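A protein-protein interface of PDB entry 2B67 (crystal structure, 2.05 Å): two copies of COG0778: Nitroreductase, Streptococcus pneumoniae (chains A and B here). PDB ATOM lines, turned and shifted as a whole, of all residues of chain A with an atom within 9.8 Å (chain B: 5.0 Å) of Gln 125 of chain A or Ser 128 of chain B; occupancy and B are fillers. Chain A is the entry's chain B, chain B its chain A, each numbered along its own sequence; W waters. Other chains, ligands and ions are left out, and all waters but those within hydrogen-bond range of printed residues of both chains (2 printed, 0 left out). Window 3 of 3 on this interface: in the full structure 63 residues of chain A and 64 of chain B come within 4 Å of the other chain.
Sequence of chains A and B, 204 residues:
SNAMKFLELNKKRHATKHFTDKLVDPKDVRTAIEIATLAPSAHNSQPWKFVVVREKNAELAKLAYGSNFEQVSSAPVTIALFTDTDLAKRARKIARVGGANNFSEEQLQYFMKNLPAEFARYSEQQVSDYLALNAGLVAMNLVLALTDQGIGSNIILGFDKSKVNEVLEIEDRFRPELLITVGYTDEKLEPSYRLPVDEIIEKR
Water W2 bridges the side-chain carboxylate of Asp 129 of chain B (2.9 Å) and the side-chain amino group of Lys 161 of chain A (3.4 Å). Water W1 lies within hydrogen-bond range of the side-chain carboxylate (OD2) of Asp 129 of chain B (2.9 Å), the side-chain amino group (NZ) of Lys 161 of chain A (3.0 Å), the side-chain carboxylate (OE1) of Glu 177 of chain A (3.0 Å) and the guanidinium group (NH1) of Arg 175 of chain A (3.2 Å).
Phe 119 of chain A touches none of the printed residues of chain B. Of the printed residues of chain B, Gln 125 of chain A touches Ser 128. Of the printed residues of chain B, Arg 175 of chain A touches Gln 125 (3.9 Å) and Asp 129 (3.8 Å). Gln 126 of chain B touches none of the printed residues of chain A. No residue of chain A comes within 4 Å of Val 127 of chain B. Of chain A, only Gln 125 (3.3 Å) and Asp 129 (2.5 Å) come within 4 Å of Ser 128 of chain B. Asp 129 of chain B touches just these residues of chain A: Ser 128 (2.6 Å), Asp 129 (3.7 Å), Ala 132 (3.5 Å) and Arg 175 (3.8 Å). Of the printed residues of chain A, Tyr 130 of chain B touches Leu 157. Of the printed residues of chain A, Ala 132 of chain B touches Asp 129, Ala 132 and Leu 133. Printed residues of chain A within 4 Å of Arg 175 of chain B: Asp 129. The nearest printed residue of chain B that does not touch Gln 125 of chain A is Arg 175 of chain B (4.01 Å).
Hydrophobic or aromatic side chains of chain A that line the printed part of chain B: Ala 132, Leu 133 and Leu 157. Of the 10 printed residues of chain B, 6 touch a printed residue of chain A. Hydrophobic or aromatic side chains of chain B that line the printed part of chain A: Tyr 130 and Ala 132. Among the printed residues, Asp or Glu carboxylates within 4 Å of a Lys or Arg side-chain nitrogen of the other chain: Asp 129 of chain A with Arg 175 of chain B (3.9 Å) and Arg 175 of chain A with Asp 129 of chain B (3.8 Å).
The side-chain amide nitrogen (NE2) of Gln 125 of chain B sits at hydrogen-bond distance from the side-chain carboxylate (OD2) of Asp 129 of chain B (3.1 Å). The guanidinium group of Arg 175 of chain B lies within hydrogen-bond range of the backbone carbonyl oxygen of Ser 128 of chain B (2.8 Å). OE1 of Gln 125 of chain A sits close to OD2 of Asp 129 of chain A (3.2 Å). The side-chain hydroxyl of Ser 128 of chain A is in hydrogen-bond range of the guanidinium group of Arg 175 of chain A, at 2.8 Å. The guanidinium group of Arg 175 of chain A lies within salt-bridge range of the side-chain carboxylate of Glu 177 of chain A.
The side-chain amide nitrogen (NE2) of Gln 125 of chain B is in hydrogen-bond range of the side-chain hydroxyl (OG) of Ser 128 of chain A. The side-chain hydroxyl of Ser 128 of chain B lies within hydrogen-bond range of the side-chain amide oxygen of Gln 125 of chain A, at 3.3 Å. The side-chain carboxylate (OD1) of Asp 129 of chain A lies within hydrogen-bond range of the side-chain hydroxyl (OG) of Ser 128 of chain B, 2.5 Å away. The side-chain carboxylate (OD1) of Asp 129 of chain B lies within hydrogen-bond range of the side-chain hydroxyl (OG) of Ser 128 of chain A (2.6 Å). The side-chain carboxylate (OD2) of Asp 129 of chain B lies within salt-bridge range of the guanidinium group (NH1) of Arg 175 of chain A, at 3.8 Å. NH2 of Arg 175 of chain B is in salt-bridge range of OD2 of Asp 129 of chain A.
Gln 125 of chain A touches Ser 128 of chain B, and with the chains exchanged Ser 128 of chain A touches Gln 125 of chain B. Ser 128 of chain A touches Asp 129 of chain B, and with the chains exchanged Asp 129 of chain A touches Ser 128 of chain B. Asp 129 of chain A touches Ala 132 of chain B, and with the chains exchanged Ala 132 of chain A touches Asp 129 of chain B. Arg 175 of chain A touches Gln 125 of chain B, but with the chains exchanged Gln 125 of chain A does not touch Arg 175 of chain B (4.01 Å). Of the 13 pairs that touch across the chains among the printed residues, 10 have their exchanged pair printed and touching as well.
Among the printed residues, merely in contact across the chains: Leu 133 of chain A with Ala 132 of chain B, Ala 132 of chain A with Asp 129 of chain B, Asp 129 of chain A with Ala 132 of chain B, Asp 129 of chain A with Asp 129 of chain B, Leu 157 of chain A with Tyr 130 of chain B, Ala 132 of chain A with Ala 132 of chain B and Arg 175 of chain A with Gln 125 of chain B.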
ATOM      1  N   LEU A  87       5.579  30.606  -0.086  1.00  0.00           N
ATOM      2  CA  LEU A  87       5.780  29.179   0.122  1.00  0.00           C
ATOM      3  C   LEU A  87       7.101  28.655  -0.485  1.00  0.00           C
ATOM      4  O   LEU A  87       7.739  27.747   0.070  1.00  0.00           O
ATOM      5  CB  LEU A  87       4.553  28.387  -0.355  1.00  0.00           C
ATOM      6  CG  LEU A  87       3.312  28.418   0.565  1.00  0.00           C
ATOM      7  CD1 LEU A  87       2.124  27.685  -0.091  1.00  0.00           C
ATOM      8  CD2 LEU A  87       3.622  27.796   1.924  1.00  0.00           C
ATOM      9  N   PHE A 119       4.536  25.116  -6.081  1.00  0.00           N
ATOM     10  CA  PHE A 119       3.875  26.272  -5.478  1.00  0.00           C
ATOM     11  C   PHE A 119       3.609  27.380  -6.518  1.00  0.00           C
ATOM     12  O   PHE A 119       2.597  28.054  -6.446  1.00  0.00           O
ATOM     13  CB  PHE A 119       4.669  26.822  -4.268  1.00  0.00           C
ATOM     14  CG  PHE A 119       4.632  25.926  -3.040  1.00  0.00           C
ATOM     15  CD1 PHE A 119       5.771  25.761  -2.248  1.00  0.00           C
ATOM     16  CD2 PHE A 119       3.453  25.263  -2.664  1.00  0.00           C
ATOM     17  CE1 PHE A 119       5.741  24.965  -1.078  1.00  0.00           C
ATOM     18  CE2 PHE A 119       3.409  24.443  -1.517  1.00  0.00           C
ATOM     19  CZ  PHE A 119       4.568  24.276  -0.732  1.00  0.00           C
ATOM     20  N   ARG A 121       2.583  27.202  -9.454  1.00  0.00           N
ATOM     21  CA  ARG A 121       1.445  26.870 -10.311  1.00  0.00           C
ATOM     22  C   ARG A 121       0.076  27.069  -9.616  1.00  0.00           C
ATOM     23  O   ARG A 121      -0.953  27.073 -10.273  1.00  0.00           O
ATOM     24  CB  ARG A 121       1.600  25.434 -10.862  1.00  0.00           C
ATOM     25  CG  ARG A 121       1.211  24.319  -9.897  1.00  0.00           C
ATOM     26  CD  ARG A 121       1.162  22.930 -10.605  1.00  0.00           C
ATOM     27  NE  ARG A 121       2.321  22.065 -10.401  1.00  0.00           N
ATOM     28  CZ  ARG A 121       2.308  20.946  -9.679  1.00  0.00           C
ATOM     29  NH1 ARG A 121       1.190  20.540  -9.068  1.00  0.00           N
ATOM     30  NH2 ARG A 121       3.422  20.241  -9.552  1.00  0.00           N
ATOM     31  N   TYR A 122       0.075  27.238  -8.296  1.00  0.00           N
ATOM     32  CA  TYR A 122      -1.161  27.377  -7.503  1.00  0.00           C
ATOM     33  C   TYR A 122      -1.855  28.719  -7.773  1.00  0.00           C
ATOM     34  O   TYR A 122      -1.219  29.760  -7.775  1.00  0.00           O
ATOM     35  CB  TYR A 122      -0.837  27.292  -5.991  1.00  0.00           C
ATOM     36  CG  TYR A 122      -0.477  25.921  -5.427  1.00  0.00           C
ATOM     37  CD1 TYR A 122      -0.133  24.834  -6.266  1.00  0.00           C
ATOM     38  CD2 TYR A 122      -0.456  25.703  -4.037  1.00  0.00           C
ATOM     39  CE1 TYR A 122       0.183  23.571  -5.729  1.00  0.00           C
ATOM     40  CE2 TYR A 122      -0.136  24.434  -3.500  1.00  0.00           C
ATOM     41  CZ  TYR A 122       0.198  23.388  -4.343  1.00  0.00           C
ATOM     42  OH  TYR A 122       0.524  22.138  -3.815  1.00  0.00           O
ATOM     43  N   SER A 123      -3.165  28.692  -7.981  1.00  0.00           N
ATOM     44  CA  SER A 123      -3.952  29.924  -7.982  1.00  0.00           C
ATOM     45  C   SER A 123      -3.864  30.618  -6.614  1.00  0.00           C
ATOM     46  O   SER A 123      -3.437  30.010  -5.605  1.00  0.00           O
ATOM     47  CB  SER A 123      -5.408  29.611  -8.297  1.00  0.00           C
ATOM     48  OG  SER A 123      -5.995  28.846  -7.253  1.00  0.00           O
ATOM     49  N   GLU A 124      -4.245  31.893  -6.588  1.00  0.00           N
ATOM     50  CA  GLU A 124      -4.347  32.668  -5.363  1.00  0.00           C
ATOM     51  C   GLU A 124      -5.223  31.967  -4.291  1.00  0.00           C
ATOM     52  O   GLU A 124      -4.816  31.896  -3.142  1.00  0.00           O
ATOM     53  CB  GLU A 124      -4.954  34.034  -5.660  1.00  0.00           C
ATOM     54  CG  GLU A 124      -4.044  34.974  -6.437  1.00  0.00           C
ATOM     55  CD  GLU A 124      -4.632  36.391  -6.538  1.00  0.00           C
ATOM     56  OE1 GLU A 124      -5.760  36.620  -6.002  1.00  0.00           O
ATOM     57  OE2 GLU A 124      -3.958  37.265  -7.161  1.00  0.00           O
ATOM     58  N   GLN A 125      -6.391  31.453  -4.691  1.00  0.00           N
ATOM     59  CA  GLN A 125      -7.311  30.753  -3.771  1.00  0.00           C
ATOM     60  C   GLN A 125      -6.697  29.452  -3.237  1.00  0.00           C
ATOM     61  O   GLN A 125      -6.832  29.124  -2.066  1.00  0.00           O
ATOM     62  CB  GLN A 125      -8.647  30.418  -4.453  1.00  0.00           C
ATOM     63  CG  GLN A 125      -9.701  29.854  -3.477  1.00  0.00           C
ATOM     64  CD  GLN A 125     -10.775  28.975  -4.131  1.00  0.00           C
ATOM     65  OE1 GLN A 125     -11.099  27.884  -3.623  1.00  0.00           O
ATOM     66  NE2 GLN A 125     -11.331  29.439  -5.246  1.00  0.00           N
ATOM     67  N   GLN A 126      -6.037  28.716  -4.120  1.00  0.00           N
ATOM     68  CA  GLN A 126      -5.376  27.488  -3.751  1.00  0.00           C
ATOM     69  C   GLN A 126      -4.315  27.744  -2.684  1.00  0.00           C
ATOM     70  O   GLN A 126      -4.262  27.032  -1.673  1.00  0.00           O
ATOM     71  CB  GLN A 126      -4.755  26.812  -4.972  1.00  0.00           C
ATOM     72  CG  GLN A 126      -4.355  25.355  -4.730  1.00  0.00           C
ATOM     73  CD  GLN A 126      -3.884  24.649  -5.993  1.00  0.00           C
ATOM     74  OE1 GLN A 126      -3.485  23.471  -5.931  1.00  0.00           O
ATOM     75  NE2 GLN A 126      -3.927  25.364  -7.157  1.00  0.00           N
ATOM     76  N   VAL A 127      -3.481  28.754  -2.905  1.00  0.00           N
ATOM     77  CA  VAL A 127      -2.556  29.170  -1.890  1.00  0.00           C
ATOM     78  C   VAL A 127      -3.236  29.586  -0.573  1.00  0.00           C
ATOM     79  O   VAL A 127      -2.808  29.147   0.482  1.00  0.00           O
ATOM     80  CB  VAL A 127      -1.634  30.286  -2.349  1.00  0.00           C
ATOM     81  CG1 VAL A 127      -0.810  30.762  -1.164  1.00  0.00           C
ATOM     82  CG2 VAL A 127      -0.696  29.765  -3.487  1.00  0.00           C
ATOM     83  N   SER A 128      -4.287  30.423  -0.639  1.00  0.00           N
ATOM     84  CA  SER A 128      -5.018  30.812   0.569  1.00  0.00           C
ATOM     85  C   SER A 128      -5.592  29.609   1.338  1.00  0.00           C
ATOM     86  O   SER A 128      -5.526  29.548   2.579  1.00  0.00           O
ATOM     87  CB  SER A 128      -6.142  31.811   0.210  1.00  0.00           C
ATOM     88  OG  SER A 128      -6.525  32.603   1.332  1.00  0.00           O
ATOM     89  N   ASP A 129      -6.187  28.676   0.610  1.00  0.00           N
ATOM     90  CA  ASP A 129      -6.780  27.491   1.214  1.00  0.00           C
ATOM     91  C   ASP A 129      -5.711  26.596   1.854  1.00  0.00           C
ATOM     92  O   ASP A 129      -5.949  25.991   2.907  1.00  0.00           O
ATOM     93  CB  ASP A 129      -7.539  26.684   0.168  1.00  0.00           C
ATOM     94  CG  ASP A 129      -8.866  27.331  -0.260  1.00  0.00           C
ATOM     95  OD1 ASP A 129      -9.217  28.467   0.189  1.00  0.00           O
ATOM     96  OD2 ASP A 129      -9.552  26.661  -1.078  1.00  0.00           O
ATOM     97  N   TYR A 130      -4.545  26.516   1.202  1.00  0.00           N
ATOM     98  CA  TYR A 130      -3.386  25.711   1.680  1.00  0.00           C
ATOM     99  C   TYR A 130      -2.879  26.216   3.056  1.00  0.00           C
ATOM    100  O   TYR A 130      -2.669  25.442   3.986  1.00  0.00           O
ATOM    101  CB  TYR A 130      -2.294  25.763   0.597  1.00  0.00           C
ATOM    102  CG  TYR A 130      -1.047  24.961   0.829  1.00  0.00           C
ATOM    103  CD1 TYR A 130      -0.876  23.709   0.207  1.00  0.00           C
ATOM    104  CD2 TYR A 130       0.003  25.458   1.635  1.00  0.00           C
ATOM    105  CE1 TYR A 130       0.298  22.966   0.412  1.00  0.00           C
ATOM    106  CE2 TYR A 130       1.177  24.703   1.843  1.00  0.00           C
ATOM    107  CZ  TYR A 130       1.304  23.467   1.234  1.00  0.00           C
ATOM    108  OH  TYR A 130       2.461  22.739   1.403  1.00  0.00           O
ATOM    109  N   LEU A 131      -2.714  27.522   3.186  1.00  0.00           N
ATOM    110  CA  LEU A 131      -2.237  28.104   4.437  1.00  0.00           C
ATOM    111  C   LEU A 131      -3.299  27.940   5.522  1.00  0.00           C
ATOM    112  O   LEU A 131      -2.971  27.563   6.637  1.00  0.00           O
ATOM    113  CB  LEU A 131      -1.855  29.579   4.251  1.00  0.00           C
ATOM    114  CG  LEU A 131      -0.804  29.902   3.169  1.00  0.00           C
ATOM    115  CD1 LEU A 131      -0.625  31.405   3.135  1.00  0.00           C
ATOM    116  CD2 LEU A 131       0.537  29.218   3.445  1.00  0.00           C
ATOM    117  N   ALA A 132      -4.558  28.213   5.182  1.00  0.00           N
ATOM    118  CA  ALA A 132      -5.662  28.090   6.153  1.00  0.00           C
ATOM    119  C   ALA A 132      -5.762  26.670   6.712  1.00  0.00           C
ATOM    120  O   ALA A 132      -5.845  26.477   7.937  1.00  0.00           O
ATOM    121  CB  ALA A 132      -7.003  28.538   5.530  1.00  0.00           C
ATOM    122  N   LEU A 133      -5.711  25.677   5.823  1.00  0.00           N
ATOM    123  CA  LEU A 133      -5.829  24.281   6.266  1.00  0.00           C
ATOM    124  C   LEU A 133      -4.675  23.843   7.166  1.00  0.00           C
ATOM    125  O   LEU A 133      -4.878  23.185   8.208  1.00  0.00           O
ATOM    126  CB  LEU A 133      -5.972  23.336   5.063  1.00  0.00           C
ATOM    127  CG  LEU A 133      -6.395  21.897   5.431  1.00  0.00           C
ATOM    128  CD1 LEU A 133      -7.526  21.421   4.498  1.00  0.00           C
ATOM    129  CD2 LEU A 133      -5.158  21.044   5.323  1.00  0.00           C
ATOM    130  N   LEU A 157     -11.328  33.640  15.677  1.00  0.00           N
ATOM    131  CA  LEU A 157     -11.276  34.033  14.288  1.00  0.00           C
ATOM    132  C   LEU A 157     -11.856  35.433  14.101  1.00  0.00           C
ATOM    133  O   LEU A 157     -11.726  36.010  13.032  1.00  0.00           O
ATOM    134  CB  LEU A 157     -12.090  33.050  13.444  1.00  0.00           C
ATOM    135  CG  LEU A 157     -11.418  32.422  12.216  1.00  0.00           C
ATOM    136  CD1 LEU A 157     -12.472  31.847  11.245  1.00  0.00           C
ATOM    137  CD2 LEU A 157     -10.401  33.334  11.485  1.00  0.00           C
ATOM    138  N   LYS A 161      -7.909  41.179  10.767  1.00  0.00           N
ATOM    139  CA  LYS A 161      -6.667  40.646  10.191  1.00  0.00           C
ATOM    140  C   LYS A 161      -5.767  41.711   9.545  1.00  0.00           C
ATOM    141  O   LYS A 161      -4.541  41.553   9.515  1.00  0.00           O
ATOM    142  CB  LYS A 161      -6.972  39.543   9.169  1.00  0.00           C
ATOM    143  CG  LYS A 161      -7.403  38.203   9.773  1.00  0.00           C
ATOM    144  CD  LYS A 161      -7.790  37.198   8.670  1.00  0.00           C
ATOM    145  CE  LYS A 161      -7.884  35.765   9.212  1.00  0.00           C
ATOM    146  NZ  LYS A 161      -8.500  34.871   8.207  1.00  0.00           N
ATOM    147  N   ARG A 175       0.888  36.076   7.330  1.00  0.00           N
ATOM    148  CA  ARG A 175      -0.474  36.540   7.501  1.00  0.00           C
ATOM    149  C   ARG A 175      -1.154  35.943   8.724  1.00  0.00           C
ATOM    150  O   ARG A 175      -1.015  34.742   9.006  1.00  0.00           O
ATOM    151  CB  ARG A 175      -1.316  36.295   6.242  1.00  0.00           C
ATOM    152  CG  ARG A 175      -1.585  34.824   5.939  1.00  0.00           C
ATOM    153  CD  ARG A 175      -2.665  34.687   4.880  1.00  0.00           C
ATOM    154  NE  ARG A 175      -3.399  33.436   5.033  1.00  0.00           N
ATOM    155  CZ  ARG A 175      -4.249  32.935   4.129  1.00  0.00           C
ATOM    156  NH1 ARG A 175      -4.861  31.773   4.384  1.00  0.00           N
ATOM    157  NH2 ARG A 175      -4.488  33.584   2.974  1.00  0.00           N
ATOM    158  N   GLU A 177      -3.660  34.159  11.005  1.00  0.00           N
ATOM    159  CA  GLU A 177      -4.728  33.176  10.786  1.00  0.00           C
ATOM    160  C   GLU A 177      -5.717  33.118  11.946  1.00  0.00           C
ATOM    161  O   GLU A 177      -6.942  33.102  11.746  1.00  0.00           O
ATOM    162  CB  GLU A 177      -4.144  31.780  10.479  1.00  0.00           C
ATOM    163  CG  GLU A 177      -3.337  31.720   9.152  1.00  0.00           C
ATOM    164  CD  GLU A 177      -4.196  31.524   7.883  1.00  0.00           C
ATOM    165  OE1 GLU A 177      -5.443  31.589   7.935  1.00  0.00           O
ATOM    166  OE2 GLU A 177      -3.616  31.314   6.800  1.00  0.00           O
ATOM    167  N   GLU B 124     -15.676  35.807  -0.862  1.00  0.00           N
ATOM    168  CA  GLU B 124     -15.402  34.459  -1.336  1.00  0.00           C
ATOM    169  C   GLU B 124     -14.130  33.842  -0.729  1.00  0.00           C
ATOM    170  O   GLU B 124     -14.103  32.637  -0.467  1.00  0.00           O
ATOM    171  CB  GLU B 124     -15.386  34.394  -2.862  1.00  0.00           C
ATOM    172  CG  GLU B 124     -16.715  33.900  -3.414  1.00  0.00           C
ATOM    173  CD  GLU B 124     -16.663  33.582  -4.895  1.00  0.00           C
ATOM    174  OE1 GLU B 124     -16.991  34.498  -5.691  1.00  0.00           O
ATOM    175  OE2 GLU B 124     -16.291  32.425  -5.251  1.00  0.00           O
ATOM    176  N   GLN B 125     -13.109  34.671  -0.489  1.00  0.00           N
ATOM    177  CA  GLN B 125     -11.875  34.216   0.127  1.00  0.00           C
ATOM    178  C   GLN B 125     -12.130  33.909   1.589  1.00  0.00           C
ATOM    179  O   GLN B 125     -11.602  32.943   2.095  1.00  0.00           O
ATOM    180  CB  GLN B 125     -10.734  35.247  -0.002  1.00  0.00           C
ATOM    181  CG  GLN B 125      -9.417  34.760   0.670  1.00  0.00           C
ATOM    182  CD  GLN B 125      -8.384  35.870   0.949  1.00  0.00           C
ATOM    183  OE1 GLN B 125      -8.259  36.825   0.173  1.00  0.00           O
ATOM    184  NE2 GLN B 125      -7.622  35.724   2.050  1.00  0.00           N
ATOM    185  N   GLN B 126     -12.938  34.737   2.257  1.00  0.00           N
ATOM    186  CA  GLN B 126     -13.254  34.521   3.673  1.00  0.00           C
ATOM    187  C   GLN B 126     -13.955  33.198   3.888  1.00  0.00           C
ATOM    188  O   GLN B 126     -13.531  32.437   4.746  1.00  0.00           O
ATOM    189  CB  GLN B 126     -14.073  35.662   4.270  1.00  0.00           C
ATOM    190  CG  GLN B 126     -13.244  36.917   4.552  1.00  0.00           C
ATOM    191  CD  GLN B 126     -14.087  38.102   5.084  1.00  0.00           C
ATOM    192  OE1 GLN B 126     -15.311  38.061   5.066  1.00  0.00           O
ATOM    193  NE2 GLN B 126     -13.414  39.134   5.594  1.00  0.00           N
ATOM    194  N   VAL B 127     -14.997  32.926   3.095  1.00  0.00           N
ATOM    195  CA  VAL B 127     -15.669  31.618   3.089  1.00  0.00           C
ATOM    196  C   VAL B 127     -14.708  30.447   2.827  1.00  0.00           C
ATOM    197  O   VAL B 127     -14.689  29.465   3.587  1.00  0.00           O
ATOM    198  CB  VAL B 127     -16.865  31.566   2.107  1.00  0.00           C
ATOM    199  CG1 VAL B 127     -17.446  30.141   2.015  1.00  0.00           C
ATOM    200  CG2 VAL B 127     -17.970  32.473   2.592  1.00  0.00           C
ATOM    201  N   SER B 128     -13.917  30.562   1.762  1.00  0.00           N
ATOM    202  CA  SER B 128     -13.034  29.488   1.349  1.00  0.00           C
ATOM    203  C   SER B 128     -11.961  29.163   2.430  1.00  0.00           C
ATOM    204  O   SER B 128     -11.644  27.983   2.660  1.00  0.00           O
ATOM    205  CB  SER B 128     -12.351  29.826   0.005  1.00  0.00           C
ATOM    206  OG  SER B 128     -11.660  28.686  -0.484  1.00  0.00           O
ATOM    207  N   ASP B 129     -11.392  30.207   3.029  1.00  0.00           N
ATOM    208  CA  ASP B 129     -10.435  30.108   4.153  1.00  0.00           C
ATOM    209  C   ASP B 129     -11.049  29.509   5.398  1.00  0.00           C
ATOM    210  O   ASP B 129     -10.400  28.718   6.115  1.00  0.00           O
ATOM    211  CB  ASP B 129      -9.826  31.483   4.513  1.00  0.00           C
ATOM    212  CG  ASP B 129      -8.823  32.006   3.441  1.00  0.00           C
ATOM    213  OD1 ASP B 129      -8.541  31.301   2.450  1.00  0.00           O
ATOM    214  OD2 ASP B 129      -8.321  33.144   3.592  1.00  0.00           O
ATOM    215  N   TYR B 130     -12.293  29.900   5.665  1.00  0.00           N
ATOM    216  CA  TYR B 130     -13.048  29.437   6.849  1.00  0.00           C
ATOM    217  C   TYR B 130     -13.239  27.914   6.762  1.00  0.00           C
ATOM    218  O   TYR B 130     -12.946  27.172   7.698  1.00  0.00           O
ATOM    219  CB  TYR B 130     -14.382  30.176   6.878  1.00  0.00           C
ATOM    220  CG  TYR B 130     -15.305  29.931   8.027  1.00  0.00           C
ATOM    221  CD1 TYR B 130     -15.393  30.847   9.084  1.00  0.00           C
ATOM    222  CD2 TYR B 130     -16.147  28.826   8.036  1.00  0.00           C
ATOM    223  CE1 TYR B 130     -16.312  30.647  10.153  1.00  0.00           C
ATOM    224  CE2 TYR B 130     -17.046  28.596   9.100  1.00  0.00           C
ATOM    225  CZ  TYR B 130     -17.157  29.522  10.132  1.00  0.00           C
ATOM    226  OH  TYR B 130     -18.069  29.260  11.180  1.00  0.00           O
ATOM    227  N   LEU B 131     -13.679  27.451   5.607  1.00  0.00           N
ATOM    228  CA  LEU B 131     -13.911  26.021   5.414  1.00  0.00           C
ATOM    229  C   LEU B 131     -12.582  25.249   5.498  1.00  0.00           C
ATOM    230  O   LEU B 131     -12.489  24.191   6.127  1.00  0.00           O
ATOM    231  CB  LEU B 131     -14.598  25.798   4.077  1.00  0.00           C
ATOM    232  CG  LEU B 131     -16.030  26.357   3.893  1.00  0.00           C
ATOM    233  CD1 LEU B 131     -16.523  26.008   2.480  1.00  0.00           C
ATOM    234  CD2 LEU B 131     -17.036  25.848   4.913  1.00  0.00           C
ATOM    235  N   ALA B 132     -11.536  25.801   4.872  1.00  0.00           N
ATOM    236  CA  ALA B 132     -10.249  25.125   4.840  1.00  0.00           C
ATOM    237  C   ALA B 132      -9.667  25.020   6.264  1.00  0.00           C
ATOM    238  O   ALA B 132      -9.115  23.975   6.664  1.00  0.00           O
ATOM    239  CB  ALA B 132      -9.268  25.831   3.879  1.00  0.00           C
ATOM    240  N   ARG B 175     -17.837  20.536  -0.682  1.00  0.00           N
ATOM    241  CA  ARG B 175     -16.603  20.479  -1.469  1.00  0.00           C
ATOM    242  C   ARG B 175     -15.549  19.606  -0.785  1.00  0.00           C
ATOM    243  O   ARG B 175     -15.426  19.612   0.458  1.00  0.00           O
ATOM    244  CB  ARG B 175     -16.037  21.866  -1.760  1.00  0.00           C
ATOM    245  CG  ARG B 175     -15.548  22.568  -0.531  1.00  0.00           C
ATOM    246  CD  ARG B 175     -14.712  23.789  -0.894  1.00  0.00           C
ATOM    247  NE  ARG B 175     -13.856  24.217   0.216  1.00  0.00           N
ATOM    248  CZ  ARG B 175     -13.209  25.388   0.250  1.00  0.00           C
ATOM    249  NH1 ARG B 175     -12.449  25.709   1.296  1.00  0.00           N
ATOM    250  NH2 ARG B 175     -13.372  26.274  -0.740  1.00  0.00           N
HETATM  251  O   HOH W   1      -6.877  33.552   6.102  1.00  0.00           O
HETATM  252  O   HOH W   2      -9.934  34.941   5.143  1.00  0.00           O
